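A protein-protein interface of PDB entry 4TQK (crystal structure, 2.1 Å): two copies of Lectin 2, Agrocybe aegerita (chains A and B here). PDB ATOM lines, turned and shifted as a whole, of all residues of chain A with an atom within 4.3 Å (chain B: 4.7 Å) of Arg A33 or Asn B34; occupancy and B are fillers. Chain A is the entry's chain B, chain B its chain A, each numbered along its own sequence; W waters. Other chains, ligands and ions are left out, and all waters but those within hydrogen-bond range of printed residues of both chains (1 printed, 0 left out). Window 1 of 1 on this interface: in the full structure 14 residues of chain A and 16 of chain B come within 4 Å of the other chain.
Water W1 lies within hydrogen-bond range of OD1 of Asp B20 (2.7 Å), O of Phe B18 (2.9 Å) and NH2 of Arg A33 (3.0 Å).
Of the 9 printed residues of chain B, 4 touch a printed residue of chain A.
Hydrophobic or aromatic side chains of chain A within 4 Å of the printed part of chain B: Ala A35 and Val A36.
Gly A32 touches none of the printed residues of chain B.
Printed residues of chain B within 4 Å of Arg A33: Phe B18 (3.4 Å), Arg B33 (3.7 Å) and Asn B34 (3.1 Å).
Of the printed residues of chain B, Asn A34 touches Arg B33, Asn B34 and Ala B35.
Of the printed residues of chain B, Ala A35 touches Phe B18 (3.6 Å), Asn B34 (3.4 Å) and Ala B35 (3.3 Å).
Of the printed residues of chain B, Val A36 touches Asn B34 (2.9 Å) and Ala B35 (3.4 Å).
Ala B19 touches none of the printed residues of chain A.
Printed residues of chain A within 4 Å of Arg B33: Arg A33 (3.7 Å) and Asn A34 (3.7 Å).
Of chain A, only Arg A33 (3.1 Å), Asn A34 (3.4 Å), Ala A35 (3.4 Å) and Val A36 (2.9 Å) come within 4 Å of Asn B34.
Printed residues of chain A within 4 Å of Ala B35: Asn A34 (3.2 Å), Ala A35 (3.3 Å) and Val A36 (3.4 Å).
The nearest printed residue of chain B that does not touch Arg A33 is Ala B35 (5.0 Å).
The nearest printed residue of chain A that does not touch Arg B33 is Asp A402 (4.8 Å).
Among the printed residues, pairs that only touch across the chains: Arg A33 with Phe B18 (3.4 Å), Arg A33 with Arg B33 (3.7 Å), Asn A34 with Arg B33 (3.7 Å), Asn A34 with Ala B35 (3.2 Å), Ala A35 with Phe B18 (3.6 Å), Ala A35 with Asn B34 (3.4 Å) and Ala A35 with Ala B35 (3.3 Å).
O of Asn B34 sits at hydrogen-bond distance from NH2 of Arg A33 (3.1 Å).
N of Val A36 is in hydrogen-bond range of OD1 of Asn B34 (2.9 Å).
O of Asn A34 sits close to O of Asn B34.
The backbone NH (N) of Val A36 sits close to the backbone carbonyl oxygen (O) of Ala B35 (3.4 Å).
N of Asn B34 lies within hydrogen-bond range of OD1 of Asp B20 (2.8 Å).
The side-chain carboxylate (OD1) of Asp A402 lies within salt-bridge range of the guanidinium group (NH1) of Arg A33, at 3.5 Å.
The side-chain amide nitrogen (ND2) of Asn B34 is in hydrogen-bond range of the backbone carbonyl oxygen (O) of Leu B345 (3.2 Å).
The side-chain amide nitrogen of Asn B34 sits at hydrogen-bond distance from the backbone carbonyl oxygen of Ala B19.
N of Asn A34 is in hydrogen-bond range of OD1 of Asp A20, at 2.6 Å.
NE of Arg A33 is in salt-bridge range of OD1 of Asp A20, 3.8 Å away.
Arg A33 touches its own counterpart, Arg B33.
Arg A33 touches Asn B34, and with the chains exchanged Asn A34 touches Arg B33.
Asn A34 touches its own counterpart, Asn B34.
Asn A34 touches Ala B35, and with the chains exchanged Ala A35 touches Asn B34.
Of the 11 pairs that touch across the chains among the printed residues, 7 have their exchanged pair printed and touching as well.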
ATOM      1  N   ASP A  20     -19.662 -10.453  -7.960  1.00  0.00           N
ATOM      2  CA  ASP A  20     -18.368 -11.061  -8.275  1.00  0.00           C
ATOM      3  C   ASP A  20     -17.382  -9.986  -8.714  1.00  0.00           C
ATOM      4  O   ASP A  20     -17.795  -8.911  -9.155  1.00  0.00           O
ATOM      5  CB  ASP A  20     -18.508 -12.097  -9.397  1.00  0.00           C
ATOM      6  CG  ASP A  20     -19.412 -13.250  -9.017  1.00  0.00           C
ATOM      7  OD1 ASP A  20     -19.078 -13.980  -8.071  1.00  0.00           O
ATOM      8  OD2 ASP A  20     -20.456 -13.437  -9.658  1.00  0.00           O
ATOM      9  N   ILE A  31     -10.969 -13.289 -12.958  1.00  0.00           N
ATOM     10  CA  ILE A  31     -12.241 -13.425 -12.255  1.00  0.00           C
ATOM     11  C   ILE A  31     -12.046 -13.782 -10.786  1.00  0.00           C
ATOM     12  O   ILE A  31     -11.314 -14.721 -10.460  1.00  0.00           O
ATOM     13  CB  ILE A  31     -13.095 -14.556 -12.870  1.00  0.00           C
ATOM     14  CG1 ILE A  31     -13.194 -14.418 -14.399  1.00  0.00           C
ATOM     15  CG2 ILE A  31     -14.452 -14.656 -12.159  1.00  0.00           C
ATOM     16  CD1 ILE A  31     -13.949 -13.195 -14.885  1.00  0.00           C
ATOM     17  N   GLY A  32     -12.723 -13.047  -9.907  1.00  0.00           N
ATOM     18  CA  GLY A  32     -12.822 -13.424  -8.506  1.00  0.00           C
ATOM     19  C   GLY A  32     -14.268 -13.728  -8.166  1.00  0.00           C
ATOM     20  O   GLY A  32     -15.002 -12.852  -7.710  1.00  0.00           O
ATOM     21  N   ARG A  33     -14.692 -14.961  -8.435  1.00  0.00           N
ATOM     22  CA  ARG A  33     -16.031 -15.430  -8.089  1.00  0.00           C
ATOM     23  C   ARG A  33     -16.255 -15.255  -6.587  1.00  0.00           C
ATOM     24  O   ARG A  33     -15.441 -15.709  -5.788  1.00  0.00           O
ATOM     25  CB  ARG A  33     -16.154 -16.925  -8.419  1.00  0.00           C
ATOM     26  CG  ARG A  33     -17.336 -17.353  -9.295  1.00  0.00           C
ATOM     27  CD  ARG A  33     -18.735 -17.134  -8.693  1.00  0.00           C
ATOM     28  NE  ARG A  33     -18.967 -17.734  -7.380  1.00  0.00           N
ATOM     29  CZ  ARG A  33     -20.081 -18.378  -7.017  1.00  0.00           C
ATOM     30  NH1 ARG A  33     -21.079 -18.561  -7.861  1.00  0.00           N
ATOM     31  NH2 ARG A  33     -20.195 -18.858  -5.792  1.00  0.00           N
ATOM     32  N   ASN A  34     -17.351 -14.612  -6.204  1.00  0.00           N
ATOM     33  CA  ASN A  34     -17.748 -14.553  -4.797  1.00  0.00           C
ATOM     34  C   ASN A  34     -17.969 -15.982  -4.293  1.00  0.00           C
ATOM     35  O   ASN A  34     -18.925 -16.647  -4.706  1.00  0.00           O
ATOM     36  CB  ASN A  34     -19.036 -13.738  -4.668  1.00  0.00           C
ATOM     37  CG  ASN A  34     -19.285 -13.249  -3.254  1.00  0.00           C
ATOM     38  OD1 ASN A  34     -19.145 -13.995  -2.292  1.00  0.00           O
ATOM     39  ND2 ASN A  34     -19.661 -11.983  -3.127  1.00  0.00           N
ATOM     40  N   ALA A  35     -17.087 -16.463  -3.425  1.00  0.00           N
ATOM     41  CA  ALA A  35     -17.071 -17.880  -3.049  1.00  0.00           C
ATOM     42  C   ALA A  35     -16.338 -18.098  -1.723  1.00  0.00           C
ATOM     43  O   ALA A  35     -15.596 -17.221  -1.276  1.00  0.00           O
ATOM     44  CB  ALA A  35     -16.417 -18.702  -4.150  1.00  0.00           C
ATOM     45  N   VAL A  36     -16.532 -19.270  -1.112  1.00  0.00           N
ATOM     46  CA  VAL A  36     -16.009 -19.543   0.233  1.00  0.00           C
ATOM     47  C   VAL A  36     -14.484 -19.471   0.291  1.00  0.00           C
ATOM     48  O   VAL A  36     -13.897 -19.128   1.316  1.00  0.00           O
ATOM     49  CB  VAL A  36     -16.485 -20.918   0.776  1.00  0.00           C
ATOM     50  CG1 VAL A  36     -17.950 -20.866   1.147  1.00  0.00           C
ATOM     51  CG2 VAL A  36     -16.239 -22.011  -0.248  1.00  0.00           C
ATOM     52  N   LEU A  38     -11.935 -17.545  -1.988  1.00  0.00           N
ATOM     53  CA  LEU A  38     -11.672 -16.618  -3.088  1.00  0.00           C
ATOM     54  C   LEU A  38     -10.368 -16.976  -3.795  1.00  0.00           C
ATOM     55  O   LEU A  38      -9.317 -17.030  -3.173  1.00  0.00           O
ATOM     56  CB  LEU A  38     -11.581 -15.180  -2.561  1.00  0.00           C
ATOM     57  CG  LEU A  38     -12.143 -14.009  -3.375  1.00  0.00           C
ATOM     58  CD1 LEU A  38     -11.399 -12.704  -3.026  1.00  0.00           C
ATOM     59  CD2 LEU A  38     -12.109 -14.264  -4.867  1.00  0.00           C
ATOM     60  N   ASP A 402     -23.783 -14.623 -12.246  1.00  0.00           N
ATOM     61  CA  ASP A 402     -25.058 -15.357 -12.317  1.00  0.00           C
ATOM     62  C   ASP A 402     -26.293 -14.462 -12.207  1.00  0.00           C
ATOM     63  O   ASP A 402     -26.590 -13.942 -11.133  1.00  0.00           O
ATOM     64  CB  ASP A 402     -25.138 -16.406 -11.218  1.00  0.00           C
ATOM     65  CG  ASP A 402     -23.903 -17.237 -11.136  1.00  0.00           C
ATOM     66  OD1 ASP A 402     -23.107 -16.993 -10.208  1.00  0.00           O
ATOM     67  OD2 ASP A 402     -23.719 -18.121 -12.001  1.00  0.00           O
ATOM     68  N   PHE B  18     -19.812 -24.018  -7.965  1.00  0.00           N
ATOM     69  CA  PHE B  18     -19.742 -23.601  -6.582  1.00  0.00           C
ATOM     70  C   PHE B  18     -20.983 -24.053  -5.830  1.00  0.00           C
ATOM     71  O   PHE B  18     -21.976 -23.326  -5.757  1.00  0.00           O
ATOM     72  CB  PHE B  18     -19.612 -22.081  -6.517  1.00  0.00           C
ATOM     73  CG  PHE B  18     -18.440 -21.537  -7.292  1.00  0.00           C
ATOM     74  CD1 PHE B  18     -17.268 -21.193  -6.638  1.00  0.00           C
ATOM     75  CD2 PHE B  18     -18.514 -21.374  -8.668  1.00  0.00           C
ATOM     76  CE1 PHE B  18     -16.184 -20.698  -7.338  1.00  0.00           C
ATOM     77  CE2 PHE B  18     -17.436 -20.868  -9.380  1.00  0.00           C
ATOM     78  CZ  PHE B  18     -16.265 -20.530  -8.712  1.00  0.00           C
ATOM     79  N   ALA B  19     -20.921 -25.254  -5.256  1.00  0.00           N
ATOM     80  CA  ALA B  19     -22.077 -25.829  -4.575  1.00  0.00           C
ATOM     81  C   ALA B  19     -22.444 -25.062  -3.301  1.00  0.00           C
ATOM     82  O   ALA B  19     -21.575 -24.731  -2.486  1.00  0.00           O
ATOM     83  CB  ALA B  19     -21.842 -27.278  -4.275  1.00  0.00           C
ATOM     84  N   ASP B  20     -23.741 -24.790  -3.148  1.00  0.00           N
ATOM     85  CA  ASP B  20     -24.290 -24.077  -1.993  1.00  0.00           C
ATOM     86  C   ASP B  20     -24.792 -25.069  -0.961  1.00  0.00           C
ATOM     87  O   ASP B  20     -25.030 -26.232  -1.273  1.00  0.00           O
ATOM     88  CB  ASP B  20     -25.467 -23.212  -2.424  1.00  0.00           C
ATOM     89  CG  ASP B  20     -25.110 -22.262  -3.537  1.00  0.00           C
ATOM     90  OD1 ASP B  20     -24.171 -21.467  -3.356  1.00  0.00           O
ATOM     91  OD2 ASP B  20     -25.766 -22.320  -4.593  1.00  0.00           O
ATOM     92  N   GLY B  32     -27.256 -21.606   2.824  1.00  0.00           N
ATOM     93  CA  GLY B  32     -25.834 -21.342   2.982  1.00  0.00           C
ATOM     94  C   GLY B  32     -25.156 -21.118   1.637  1.00  0.00           C
ATOM     95  O   GLY B  32     -24.478 -21.998   1.108  1.00  0.00           O
ATOM     96  N   ARG B  33     -25.337 -19.920   1.086  1.00  0.00           N
ATOM     97  CA  ARG B  33     -24.903 -19.606  -0.265  1.00  0.00           C
ATOM     98  C   ARG B  33     -23.382 -19.573  -0.317  1.00  0.00           C
ATOM     99  O   ARG B  33     -22.735 -18.857   0.456  1.00  0.00           O
ATOM    100  CB  ARG B  33     -25.418 -18.239  -0.679  1.00  0.00           C
ATOM    101  CG  ARG B  33     -26.104 -18.236  -2.035  1.00  0.00           C
ATOM    102  CD  ARG B  33     -25.199 -18.600  -3.188  1.00  0.00           C
ATOM    103  NE  ARG B  33     -24.050 -17.705  -3.389  1.00  0.00           N
ATOM    104  CZ  ARG B  33     -23.699 -17.144  -4.548  1.00  0.00           C
ATOM    105  NH1 ARG B  33     -24.406 -17.361  -5.623  1.00  0.00           N
ATOM    106  NH2 ARG B  33     -22.626 -16.375  -4.633  1.00  0.00           N
ATOM    107  N   ASN B  34     -22.812 -20.331  -1.245  1.00  0.00           N
ATOM    108  CA  ASN B  34     -21.374 -20.330  -1.431  1.00  0.00           C
ATOM    109  C   ASN B  34     -20.902 -18.915  -1.754  1.00  0.00           C
ATOM    110  O   ASN B  34     -21.123 -18.421  -2.863  1.00  0.00           O
ATOM    111  CB  ASN B  34     -21.010 -21.293  -2.552  1.00  0.00           C
ATOM    112  CG  ASN B  34     -19.547 -21.623  -2.575  1.00  0.00           C
ATOM    113  OD1 ASN B  34     -18.705 -20.746  -2.364  1.00  0.00           O
ATOM    114  ND2 ASN B  34     -19.223 -22.897  -2.828  1.00  0.00           N
ATOM    115  N   ALA B  35     -20.269 -18.259  -0.783  1.00  0.00           N
ATOM    116  CA  ALA B  35     -19.872 -16.867  -0.931  1.00  0.00           C
ATOM    117  C   ALA B  35     -18.732 -16.544   0.024  1.00  0.00           C
ATOM    118  O   ALA B  35     -18.466 -17.320   0.957  1.00  0.00           O
ATOM    119  CB  ALA B  35     -21.056 -15.957  -0.666  1.00  0.00           C
ATOM    120  N   LEU B  38     -19.723 -16.468   4.243  1.00  0.00           N
ATOM    121  CA  LEU B  38     -20.860 -17.369   4.346  1.00  0.00           C
ATOM    122  C   LEU B  38     -21.805 -16.938   5.460  1.00  0.00           C
ATOM    123  O   LEU B  38     -21.425 -16.954   6.624  1.00  0.00           O
ATOM    124  CB  LEU B  38     -20.374 -18.785   4.632  1.00  0.00           C
ATOM    125  CG  LEU B  38     -21.456 -19.844   4.460  1.00  0.00           C
ATOM    126  CD1 LEU B  38     -21.733 -20.031   2.985  1.00  0.00           C
ATOM    127  CD2 LEU B  38     -21.034 -21.153   5.117  1.00  0.00           C
ATOM    128  N   LEU B 345     -16.469 -27.002  -4.652  1.00  0.00           N
ATOM    129  CA  LEU B 345     -16.788 -25.791  -3.922  1.00  0.00           C
ATOM    130  C   LEU B 345     -16.090 -24.562  -4.505  1.00  0.00           C
ATOM    131  O   LEU B 345     -16.324 -23.445  -4.041  1.00  0.00           O
ATOM    132  CB  LEU B 345     -16.358 -25.940  -2.464  1.00  0.00           C
ATOM    133  CG  LEU B 345     -17.051 -26.985  -1.607  1.00  0.00           C
ATOM    134  CD1 LEU B 345     -16.510 -26.937  -0.187  1.00  0.00           C
ATOM    135  CD2 LEU B 345     -18.546 -26.717  -1.620  1.00  0.00           C
HETATM  136  O   HOH W   1     -22.685 -20.574  -5.418  1.00  0.00           O
